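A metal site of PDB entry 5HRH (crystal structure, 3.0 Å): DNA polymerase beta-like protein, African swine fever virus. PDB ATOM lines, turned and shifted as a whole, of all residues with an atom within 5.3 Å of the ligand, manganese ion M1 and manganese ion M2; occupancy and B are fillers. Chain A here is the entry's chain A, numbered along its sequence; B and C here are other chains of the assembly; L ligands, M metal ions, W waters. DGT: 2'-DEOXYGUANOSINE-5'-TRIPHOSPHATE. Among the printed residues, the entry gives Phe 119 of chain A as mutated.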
ATOM      1  N   VAL A  41       3.718   8.077 -19.043  1.00  0.00           N
ATOM      2  CA  VAL A  41       2.805   7.975 -17.921  1.00  0.00           C
ATOM      3  C   VAL A  41       3.555   8.409 -16.673  1.00  0.00           C
ATOM      4  O   VAL A  41       4.700   8.886 -16.740  1.00  0.00           O
ATOM      5  CB  VAL A  41       2.173   6.564 -17.747  1.00  0.00           C
ATOM      6  CG1 VAL A  41       1.167   6.259 -18.853  1.00  0.00           C
ATOM      7  CG2 VAL A  41       3.235   5.462 -17.681  1.00  0.00           C
ATOM      8  N   GLY A  42       2.883   8.284 -15.517  1.00  0.00           N
ATOM      9  CA  GLY A  42       3.453   8.724 -14.258  1.00  0.00           C
ATOM     10  C   GLY A  42       3.545  10.240 -14.124  1.00  0.00           C
ATOM     11  O   GLY A  42       2.805  11.022 -14.759  1.00  0.00           O
ATOM     12  N   SER A  43       4.474  10.668 -13.261  1.00  0.00           N
ATOM     13  CA  SER A  43       4.600  12.086 -12.980  1.00  0.00           C
ATOM     14  C   SER A  43       4.921  12.895 -14.224  1.00  0.00           C
ATOM     15  O   SER A  43       4.646  14.089 -14.249  1.00  0.00           O
ATOM     16  CB  SER A  43       5.657  12.324 -11.906  1.00  0.00           C
ATOM     17  OG  SER A  43       6.901  11.736 -12.248  1.00  0.00           O
ATOM     18  N   LEU A  44       5.479  12.264 -15.263  1.00  0.00           N
ATOM     19  CA  LEU A  44       5.719  12.978 -16.516  1.00  0.00           C
ATOM     20  C   LEU A  44       4.410  13.251 -17.262  1.00  0.00           C
ATOM     21  O   LEU A  44       4.241  14.325 -17.830  1.00  0.00           O
ATOM     22  CB  LEU A  44       6.692  12.205 -17.413  1.00  0.00           C
ATOM     23  CG  LEU A  44       7.181  12.990 -18.622  1.00  0.00           C
ATOM     24  CD1 LEU A  44       8.574  12.584 -18.942  1.00  0.00           C
ATOM     25  CD2 LEU A  44       6.295  12.763 -19.816  1.00  0.00           C
ATOM     26  N   ARG A  46       1.614  13.539 -15.773  1.00  0.00           N
ATOM     27  CA  ARG A  46       0.876  14.452 -14.912  1.00  0.00           C
ATOM     28  C   ARG A  46       1.525  15.827 -14.812  1.00  0.00           C
ATOM     29  O   ARG A  46       0.954  16.724 -14.191  1.00  0.00           O
ATOM     30  CB  ARG A  46       0.737  13.883 -13.491  1.00  0.00           C
ATOM     31  CG  ARG A  46      -0.093  12.622 -13.354  1.00  0.00           C
ATOM     32  CD  ARG A  46      -0.493  12.471 -11.905  1.00  0.00           C
ATOM     33  NE  ARG A  46       0.675  12.608 -11.035  1.00  0.00           N
ATOM     34  CZ  ARG A  46       1.510  11.644 -10.688  1.00  0.00           C
ATOM     35  NH1 ARG A  46       1.281  10.406 -11.090  1.00  0.00           N
ATOM     36  NH2 ARG A  46       2.546  11.928  -9.916  1.00  0.00           N
ATOM     37  N   MET A  50       8.991  18.305 -11.119  1.00  0.00           N
ATOM     38  CA  MET A  50      10.172  17.483 -10.918  1.00  0.00           C
ATOM     39  C   MET A  50       9.781  16.015 -10.777  1.00  0.00           C
ATOM     40  O   MET A  50       8.821  15.667 -10.119  1.00  0.00           O
ATOM     41  CB  MET A  50      11.003  17.982  -9.738  1.00  0.00           C
ATOM     42  N   LEU A  51      10.552  15.170 -11.444  1.00  0.00           N
ATOM     43  CA  LEU A  51      10.331  13.728 -11.542  1.00  0.00           C
ATOM     44  C   LEU A  51      11.420  12.991 -10.759  1.00  0.00           C
ATOM     45  O   LEU A  51      12.469  13.555 -10.452  1.00  0.00           O
ATOM     46  CB  LEU A  51      10.386  13.342 -13.027  1.00  0.00           C
ATOM     47  CG  LEU A  51       9.672  14.274 -14.026  1.00  0.00           C
ATOM     48  CD1 LEU A  51       9.968  13.932 -15.474  1.00  0.00           C
ATOM     49  CD2 LEU A  51       8.174  14.207 -13.833  1.00  0.00           C
ATOM     50  N   ASN A  52      11.183  11.711 -10.428  1.00  0.00           N
ATOM     51  CA  ASN A  52      12.329  10.910  -9.988  1.00  0.00           C
ATOM     52  C   ASN A  52      12.436   9.587 -10.727  1.00  0.00           C
ATOM     53  O   ASN A  52      13.184   8.698 -10.280  1.00  0.00           O
ATOM     54  CB  ASN A  52      12.350  10.640  -8.464  1.00  0.00           C
ATOM     55  CG  ASN A  52      10.997  10.244  -7.904  1.00  0.00           C
ATOM     56  OD1 ASN A  52      10.121  11.067  -7.732  1.00  0.00           O
ATOM     57  ND2 ASN A  52      10.844   8.979  -7.587  1.00  0.00           N
ATOM     58  N   ASP A  53      11.713   9.414 -11.831  1.00  0.00           N
ATOM     59  CA  ASP A  53      12.015   8.449 -12.881  1.00  0.00           C
ATOM     60  C   ASP A  53      11.108   8.774 -14.061  1.00  0.00           C
ATOM     61  O   ASP A  53      10.199   9.606 -13.959  1.00  0.00           O
ATOM     62  CB  ASP A  53      11.851   6.985 -12.413  1.00  0.00           C
ATOM     63  CG  ASP A  53      10.403   6.602 -12.091  1.00  0.00           C
ATOM     64  OD1 ASP A  53       9.532   7.502 -12.073  1.00  0.00           O
ATOM     65  OD2 ASP A  53      10.128   5.401 -11.849  1.00  0.00           O
ATOM     66  N   VAL A  54      11.374   8.126 -15.190  1.00  0.00           N
ATOM     67  CA  VAL A  54      10.461   8.135 -16.333  1.00  0.00           C
ATOM     68  C   VAL A  54       9.735   6.806 -16.371  1.00  0.00           C
ATOM     69  O   VAL A  54      10.349   5.748 -16.205  1.00  0.00           O
ATOM     70  CB  VAL A  54      11.196   8.398 -17.656  1.00  0.00           C
ATOM     71  CG1 VAL A  54      10.278   8.092 -18.819  1.00  0.00           C
ATOM     72  CG2 VAL A  54      11.614   9.829 -17.733  1.00  0.00           C
ATOM     73  N   ASP A  55       8.416   6.858 -16.571  1.00  0.00           N
ATOM     74  CA  ASP A  55       7.591   5.666 -16.661  1.00  0.00           C
ATOM     75  C   ASP A  55       7.000   5.636 -18.059  1.00  0.00           C
ATOM     76  O   ASP A  55       6.099   6.439 -18.368  1.00  0.00           O
ATOM     77  CB  ASP A  55       6.478   5.670 -15.601  1.00  0.00           C
ATOM     78  CG  ASP A  55       7.010   5.632 -14.181  1.00  0.00           C
ATOM     79  OD1 ASP A  55       8.036   4.962 -13.927  1.00  0.00           O
ATOM     80  OD2 ASP A  55       6.358   6.283 -13.307  1.00  0.00           O
ATOM     81  N   GLN A 102      16.534   6.691 -13.741  1.00  0.00           N
ATOM     82  CA  GLN A 102      15.731   5.476 -13.690  1.00  0.00           C
ATOM     83  C   GLN A 102      14.601   5.496 -14.719  1.00  0.00           C
ATOM     84  O   GLN A 102      13.771   6.413 -14.730  1.00  0.00           O
ATOM     85  CB  GLN A 102      15.140   5.282 -12.282  1.00  0.00           C
ATOM     86  CG  GLN A 102      14.173   4.122 -12.153  1.00  0.00           C
ATOM     87  CD  GLN A 102      13.757   3.868 -10.708  1.00  0.00           C
ATOM     88  OE1 GLN A 102      14.472   4.219  -9.769  1.00  0.00           O
ATOM     89  NE2 GLN A 102      12.568   3.303 -10.524  1.00  0.00           N
ATOM     90  N   ASP A 104      11.381   3.170 -15.972  1.00  0.00           N
ATOM     91  CA  ASP A 104      10.485   2.045 -15.719  1.00  0.00           C
ATOM     92  C   ASP A 104       9.616   1.823 -16.955  1.00  0.00           C
ATOM     93  O   ASP A 104       8.949   2.751 -17.413  1.00  0.00           O
ATOM     94  CB  ASP A 104       9.608   2.269 -14.496  1.00  0.00           C
ATOM     95  CG  ASP A 104      10.414   2.311 -13.234  1.00  0.00           C
ATOM     96  OD1 ASP A 104      11.596   1.956 -13.288  1.00  0.00           O
ATOM     97  OD2 ASP A 104       9.871   2.720 -12.181  1.00  0.00           O
ATOM     98  N   PHE A 106       6.597  -0.593 -18.835  1.00  0.00           N
ATOM     99  CA  PHE A 106       5.512  -1.528 -18.605  1.00  0.00           C
ATOM    100  C   PHE A 106       4.902  -1.899 -19.935  1.00  0.00           C
ATOM    101  O   PHE A 106       5.187  -1.292 -20.975  1.00  0.00           O
ATOM    102  CB  PHE A 106       4.421  -0.955 -17.643  1.00  0.00           C
ATOM    103  CG  PHE A 106       4.963  -0.440 -16.333  1.00  0.00           C
ATOM    104  CD1 PHE A 106       5.680   0.751 -16.271  1.00  0.00           C
ATOM    105  CD2 PHE A 106       4.951  -1.275 -15.222  1.00  0.00           C
ATOM    106  CE1 PHE A 106       6.218   1.174 -15.085  1.00  0.00           C
ATOM    107  CE2 PHE A 106       5.505  -0.879 -14.037  1.00  0.00           C
ATOM    108  CZ  PHE A 106       6.141   0.342 -13.970  1.00  0.00           C
ATOM    109  N   PHE A 119      -4.294   3.459 -14.667  1.00  0.00           N
ATOM    110  CA  PHE A 119      -3.578   2.961 -13.509  1.00  0.00           C
ATOM    111  C   PHE A 119      -2.142   3.519 -13.451  1.00  0.00           C
ATOM    112  O   PHE A 119      -1.654   3.869 -12.361  1.00  0.00           O
ATOM    113  CB  PHE A 119      -3.551   1.436 -13.573  1.00  0.00           C
ATOM    114  CG  PHE A 119      -2.719   0.801 -12.536  1.00  0.00           C
ATOM    115  CD1 PHE A 119      -3.250   0.571 -11.268  1.00  0.00           C
ATOM    116  CD2 PHE A 119      -1.369   0.536 -12.769  1.00  0.00           C
ATOM    117  CE1 PHE A 119      -2.479  -0.012 -10.268  1.00  0.00           C
ATOM    118  CE2 PHE A 119      -0.570  -0.024 -11.774  1.00  0.00           C
ATOM    119  CZ  PHE A 119      -1.126  -0.303 -10.528  1.00  0.00           C
ATOM    120  N   PHE A 120      -1.457   3.635 -14.599  1.00  0.00           N
ATOM    121  CA  PHE A 120      -0.035   3.993 -14.624  1.00  0.00           C
ATOM    122  C   PHE A 120       0.258   5.478 -14.758  1.00  0.00           C
ATOM    123  O   PHE A 120       1.444   5.854 -14.714  1.00  0.00           O
ATOM    124  CB  PHE A 120       0.710   3.254 -15.757  1.00  0.00           C
ATOM    125  CG  PHE A 120       1.077   1.851 -15.396  1.00  0.00           C
ATOM    126  CD1 PHE A 120       1.992   1.617 -14.394  1.00  0.00           C
ATOM    127  CD2 PHE A 120       0.507   0.783 -16.052  1.00  0.00           C
ATOM    128  CE1 PHE A 120       2.309   0.350 -14.032  1.00  0.00           C
ATOM    129  CE2 PHE A 120       0.826  -0.508 -15.692  1.00  0.00           C
ATOM    130  CZ  PHE A 120       1.716  -0.725 -14.684  1.00  0.00           C
ATOM    131  N   THR A 121      -0.743   6.359 -14.967  1.00  0.00           N
ATOM    132  CA  THR A 121      -0.432   7.788 -14.781  1.00  0.00           C
ATOM    133  C   THR A 121      -0.495   8.169 -13.300  1.00  0.00           C
ATOM    134  O   THR A 121       0.365   8.904 -12.805  1.00  0.00           O
ATOM    135  CB  THR A 121      -1.353   8.716 -15.592  1.00  0.00           C
ATOM    136  OG1 THR A 121      -2.650   8.765 -15.010  1.00  0.00           O
ATOM    137  CG2 THR A 121      -1.543   8.155 -16.923  1.00  0.00           C
ATOM    138  N   GLY A 122      -1.475   7.641 -12.574  1.00  0.00           N
ATOM    139  CA  GLY A 122      -1.657   8.006 -11.190  1.00  0.00           C
ATOM    140  C   GLY A 122      -2.488   9.258 -10.949  1.00  0.00           C
ATOM    141  O   GLY A 122      -3.472   9.501 -11.677  1.00  0.00           O
ATOM    142  N   PRO A 123      -2.147  10.019  -9.888  1.00  0.00           N
ATOM    143  CA  PRO A 123      -1.102   9.720  -8.881  1.00  0.00           C
ATOM    144  C   PRO A 123      -1.503   8.521  -7.992  1.00  0.00           C
ATOM    145  O   PRO A 123      -2.557   7.948  -8.200  1.00  0.00           O
ATOM    146  CB  PRO A 123      -0.997  11.017  -8.091  1.00  0.00           C
ATOM    147  CG  PRO A 123      -2.318  11.616  -8.208  1.00  0.00           C
ATOM    148  CD  PRO A 123      -2.867  11.260  -9.556  1.00  0.00           C
ATOM    149  N   VAL A 124      -0.651   8.130  -7.043  1.00  0.00           N
ATOM    150  CA  VAL A 124      -0.951   6.925  -6.260  1.00  0.00           C
ATOM    151  C   VAL A 124      -2.265   7.075  -5.494  1.00  0.00           C
ATOM    152  O   VAL A 124      -3.164   6.232  -5.590  1.00  0.00           O
ATOM    153  CB  VAL A 124       0.206   6.601  -5.309  1.00  0.00           C
ATOM    154  CG1 VAL A 124       0.066   5.220  -4.777  1.00  0.00           C
ATOM    155  CG2 VAL A 124       1.534   6.844  -6.008  1.00  0.00           C
ATOM    156  N   LEU A 127      -5.378   6.574  -7.165  1.00  0.00           N
ATOM    157  CA  LEU A 127      -5.667   5.173  -7.460  1.00  0.00           C
ATOM    158  C   LEU A 127      -6.224   4.469  -6.249  1.00  0.00           C
ATOM    159  O   LEU A 127      -7.198   3.707  -6.356  1.00  0.00           O
ATOM    160  CB  LEU A 127      -4.392   4.457  -7.907  1.00  0.00           C
ATOM    161  CG  LEU A 127      -4.077   4.357  -9.385  1.00  0.00           C
ATOM    162  CD1 LEU A 127      -4.051   5.711  -9.984  1.00  0.00           C
ATOM    163  CD2 LEU A 127      -2.706   3.707  -9.477  1.00  0.00           C
ATOM    164  P    DG B   9      -8.628  -0.540   0.688  1.00  0.00           P
ATOM    165  OP1  DG B   9      -9.450  -1.775   0.668  1.00  0.00           O
ATOM    166  OP2  DG B   9      -7.195  -0.517   1.112  1.00  0.00           O
ATOM    167  O5'  DG B   9      -8.784  -0.096  -0.825  1.00  0.00           O
ATOM    168  C5'  DG B   9      -7.706   0.415  -1.558  1.00  0.00           C
ATOM    169  C4'  DG B   9      -7.731  -0.222  -2.920  1.00  0.00           C
ATOM    170  O4'  DG B   9      -6.525   0.090  -3.621  1.00  0.00           O
ATOM    171  C3'  DG B   9      -7.799  -1.742  -2.890  1.00  0.00           C
ATOM    172  O3'  DG B   9      -8.412  -2.244  -4.087  1.00  0.00           O
ATOM    173  C2'  DG B   9      -6.313  -2.121  -2.749  1.00  0.00           C
ATOM    174  C1'  DG B   9      -5.616  -0.986  -3.515  1.00  0.00           C
ATOM    175  N9   DG B   9      -4.394  -0.468  -2.917  1.00  0.00           N
ATOM    176  C8   DG B   9      -4.140  -0.201  -1.595  1.00  0.00           C
ATOM    177  N7   DG B   9      -2.949   0.305  -1.394  1.00  0.00           N
ATOM    178  C5   DG B   9      -2.388   0.381  -2.653  1.00  0.00           C
ATOM    179  C6   DG B   9      -1.105   0.830  -3.066  1.00  0.00           C
ATOM    180  O6   DG B   9      -0.185   1.271  -2.359  1.00  0.00           O
ATOM    181  N1   DG B   9      -0.950   0.731  -4.463  1.00  0.00           N
ATOM    182  C2   DG B   9      -1.927   0.255  -5.326  1.00  0.00           C
ATOM    183  N2   DG B   9      -1.622   0.220  -6.617  1.00  0.00           N
ATOM    184  N3   DG B   9      -3.114  -0.159  -4.949  1.00  0.00           N
ATOM    185  C4   DG B   9      -3.271  -0.076  -3.608  1.00  0.00           C
ATOM    186  P    DT B  10      -8.526  -3.831  -4.358  1.00  0.00           P
ATOM    187  OP1  DT B  10      -9.690  -4.084  -5.260  1.00  0.00           O
ATOM    188  OP2  DT B  10      -8.501  -4.585  -3.078  1.00  0.00           O
ATOM    189  O5'  DT B  10      -7.158  -4.125  -5.130  1.00  0.00           O
ATOM    190  C5'  DT B  10      -6.879  -3.435  -6.331  1.00  0.00           C
ATOM    191  C4'  DT B  10      -5.512  -3.807  -6.822  1.00  0.00           C
ATOM    192  O4'  DT B  10      -4.517  -3.158  -6.042  1.00  0.00           O
ATOM    193  C3'  DT B  10      -5.223  -5.281  -6.689  1.00  0.00           C
ATOM    194  O3'  DT B  10      -5.520  -5.893  -7.914  1.00  0.00           O
ATOM    195  C2'  DT B  10      -3.701  -5.355  -6.343  1.00  0.00           C
ATOM    196  C1'  DT B  10      -3.318  -3.892  -6.115  1.00  0.00           C
ATOM    197  N1   DT B  10      -2.565  -3.609  -4.884  1.00  0.00           N
ATOM    198  C2   DT B  10      -1.303  -3.095  -4.982  1.00  0.00           C
ATOM    199  O2   DT B  10      -0.749  -2.878  -6.044  1.00  0.00           O
ATOM    200  N3   DT B  10      -0.706  -2.797  -3.777  1.00  0.00           N
ATOM    201  C4   DT B  10      -1.260  -2.970  -2.527  1.00  0.00           C
ATOM    202  O4   DT B  10      -0.644  -2.695  -1.496  1.00  0.00           O
ATOM    203  C5   DT B  10      -2.594  -3.515  -2.504  1.00  0.00           C
ATOM    204  C7   DT B  10      -3.266  -3.758  -1.207  1.00  0.00           C
ATOM    205  C6   DT B  10      -3.180  -3.795  -3.674  1.00  0.00           C
ATOM    206  P    DA C   9      10.296   2.320  -6.502  1.00  0.00           P
ATOM    207  OP1  DA C   9      10.299   2.734  -7.927  1.00  0.00           O
ATOM    208  OP2  DA C   9      11.465   2.622  -5.641  1.00  0.00           O
ATOM    209  O5'  DA C   9       8.991   2.920  -5.800  1.00  0.00           O
ATOM    210  C5'  DA C   9       7.772   3.085  -6.538  1.00  0.00           C
ATOM    211  C4'  DA C   9       7.498   1.862  -7.391  1.00  0.00           C
ATOM    212  O4'  DA C   9       7.044   0.786  -6.532  1.00  0.00           O
ATOM    213  C3'  DA C   9       6.413   2.048  -8.446  1.00  0.00           C
ATOM    214  C2'  DA C   9       5.168   1.500  -7.759  1.00  0.00           C
ATOM    215  C1'  DA C   9       5.733   0.377  -6.904  1.00  0.00           C
ATOM    216  N9   DA C   9       4.984   0.109  -5.679  1.00  0.00           N
ATOM    217  C8   DA C   9       5.292   0.515  -4.397  1.00  0.00           C
ATOM    218  N7   DA C   9       4.420   0.124  -3.506  1.00  0.00           N
ATOM    219  C5   DA C   9       3.470  -0.579  -4.240  1.00  0.00           C
ATOM    220  C6   DA C   9       2.298  -1.246  -3.868  1.00  0.00           C
ATOM    221  N6   DA C   9       1.847  -1.318  -2.613  1.00  0.00           N
ATOM    222  N1   DA C   9       1.578  -1.849  -4.848  1.00  0.00           N
ATOM    223  C2   DA C   9       2.030  -1.778  -6.103  1.00  0.00           C
ATOM    224  N3   DA C   9       3.123  -1.178  -6.572  1.00  0.00           N
ATOM    225  C4   DA C   9       3.810  -0.591  -5.583  1.00  0.00           C
HETATM  226  PG  DGT L   1       7.381   9.859  -9.605  1.00  0.00           P
HETATM  227  O1G DGT L   1       7.631   9.536  -8.171  1.00  0.00           O
HETATM  228  O2G DGT L   1       8.140  11.105  -9.995  1.00  0.00           O
HETATM  229  O3G DGT L   1       7.888   8.760 -10.493  1.00  0.00           O
HETATM  230  O3B DGT L   1       5.800  10.037  -9.783  1.00  0.00           O
HETATM  231  PB  DGT L   1       5.023   8.739 -10.254  1.00  0.00           P
HETATM  232  O1B DGT L   1       5.469   8.450 -11.660  1.00  0.00           O
HETATM  233  O2B DGT L   1       3.524   8.758 -10.104  1.00  0.00           O
HETATM  234  O3A DGT L   1       5.746   7.677  -9.305  1.00  0.00           O
HETATM  235  PA  DGT L   1       6.100   6.186  -9.802  1.00  0.00           P
HETATM  236  O1A DGT L   1       7.400   6.167 -10.586  1.00  0.00           O
HETATM  237  O2A DGT L   1       6.120   5.274  -8.591  1.00  0.00           O
HETATM  238  O5' DGT L   1       4.831   5.853 -10.729  1.00  0.00           O
HETATM  239  C5' DGT L   1       4.433   4.529 -10.821  1.00  0.00           C
HETATM  240  C4' DGT L   1       3.014   4.497 -11.318  1.00  0.00           C
HETATM  241  O4' DGT L   1       2.537   3.251 -10.875  1.00  0.00           O
HETATM  242  C3' DGT L   1       2.197   5.560 -10.649  1.00  0.00           C
HETATM  243  O3' DGT L   1       1.932   6.632 -11.512  1.00  0.00           O
HETATM  244  C2' DGT L   1       0.896   4.861 -10.302  1.00  0.00           C
HETATM  245  C1' DGT L   1       1.266   3.383 -10.288  1.00  0.00           C
HETATM  246  N9  DGT L   1       1.225   2.860  -8.919  1.00  0.00           N
HETATM  247  C8  DGT L   1       0.419   1.818  -8.558  1.00  0.00           C
HETATM  248  N7  DGT L   1       0.601   1.542  -7.246  1.00  0.00           N
HETATM  249  C5  DGT L   1       1.517   2.394  -6.769  1.00  0.00           C
HETATM  250  C6  DGT L   1       2.007   2.514  -5.497  1.00  0.00           C
HETATM  251  O6  DGT L   1       1.562   1.734  -4.628  1.00  0.00           O
HETATM  252  N1  DGT L   1       2.981   3.477  -5.250  1.00  0.00           N
HETATM  253  C2  DGT L   1       3.399   4.286  -6.280  1.00  0.00           C
HETATM  254  N2  DGT L   1       4.318   5.230  -6.052  1.00  0.00           N
HETATM  255  N3  DGT L   1       2.873   4.168  -7.557  1.00  0.00           N
HETATM  256  C4  DGT L   1       1.939   3.220  -7.801  1.00  0.00           C
HETATM  257 MN    MN M   1       8.121   4.194 -11.692  1.00  0.00          MN
HETATM  258 MN    MN M   2       7.580   8.053 -12.276  1.00  0.00          MN
HETATM  259  O   HOH W   1       8.790   4.231  -9.696  1.00  0.00           O
HETATM  260  O   HOH W   2       7.896   9.358 -13.931  1.00  0.00           O
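The side-chain carboxylate (OD2) of Asp 53 lies close to the side-chain amide nitrogen (NE2) of Gln 102. The side-chain carboxylate (OD1) of Asp 104 is in hydrogen-bond range of the side-chain amide nitrogen (NE2) of Gln 102, at 3.2 Å. The backbone carbonyl oxygen (O) of Val 54 is in hydrogen-bond range of the backbone NH (N) of Asp 104 (2.8 Å). O of Asp 55 is in hydrogen-bond range of N of Val 41 (3.0 Å). The guanidinium group (NH1) of Arg 46 sits at hydrogen-bond distance from the backbone carbonyl oxygen (O) of Thr 121, 2.5 Å away. The side-chain amide nitrogen (NE2) of Gln 102 lies within hydrogen-bond range of OP1 of DA 9 of chain C, at 3.5 Å. N1 of DA 9 of chain C sits close to N3 of DT 10 of chain B (2.7 Å). N of Gly 42 sits at hydrogen-bond distance from O of Phe 120.
N7 of DA 9 of chain C lies close to an oxygen (O6) of the ligand (3.5 Å). Residues that only touch the ligand: Gly 42 (3.3 Å), Leu 51 (3.8 Å), Phe 119 (3.3 Å), Gly 122 (3.7 Å), Val 124 (3.2 Å) and Leu 127 (3.8 Å). Hydrophobic or aromatic side chains that line the ligand: Phe 119, Phe 120, Val 124 and Leu 127. 15 residues have an atom within 4 Å of the ligand: Gly 42, Ser 43, Arg 46, Leu 51, Asn 52, Asp 53, Asp 55, Phe 119, Phe 120, Thr 121, Gly 122, Val 124, Leu 127, DG 9 of chain B and DA 9 of chain C.
An oxygen (O1B) of the ligand lies close to the backbone NH (N) of Ser 43, at 2.9 Å. O2G of the ligand lies within hydrogen-bond range of OG of Ser 43, 2.6 Å away. N2 of DG 9 of chain B lies close to N7 of the ligand, at 2.7 Å. The guanidinium group of Arg 46 lies within salt-bridge range of an oxygen (O2B) of the ligand, 3.0 Å away. The backbone NH (N) of Asn 52 is in hydrogen-bond range of an oxygen (O2G) of the ligand. OD1 of Asn 52 sits close to O1G of the ligand, at 3.0 Å. O3' of the ligand sits at hydrogen-bond distance from O of Thr 121 (3.0 Å). O of Phe 120 is in hydrogen-bond range of O3' of the ligand.
Within 4 Å of manganese ion M1: Asp 53, Asp 55 and Asp 104. Along chain A the residues within 4 Å of manganese ion M1 span positions 53 to 104.
Manganese ion M2 is bound by O3G of the ligand (1.9 Å). OD1 of Asp 53 binds manganese ion M2, at 2.0 Å. Manganese ion M2 is bound by water W2, at 2.1 Å. O1B of the ligand binds manganese ion M2 (2.2 Å). The side-chain carboxylate (OD2) of Asp 55 binds manganese ion M2 (2.4 Å). Manganese ion M2 is bound by an oxygen (O1A) of the ligand (2.5 Å). Manganese ion M2 has six donor atoms within binding distance.
Manganese ion M1 is bound by water W1 (2.1 Å), the side-chain carboxylate of Asp 104 (2.3 Å), the side-chain carboxylate of Asp 53 (2.3 Å), the side-chain carboxylate of Asp 55 (2.4 Å) and an oxygen (O1A) of the ligand (2.4 Å).
Ser 43 touches manganese ion M2 (OG to MN, 3.7 Å). Three residues have an atom within 4 Å of manganese ion M2: Ser 43, Asp 53 and Asp 55. Along chain A the residues within 4 Å of manganese ion M2 span positions 43 to 55.
Water W1 bridges OP1 of DA 9 of chain C (2.8 Å) and O2A of the ligand (3.1 Å).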
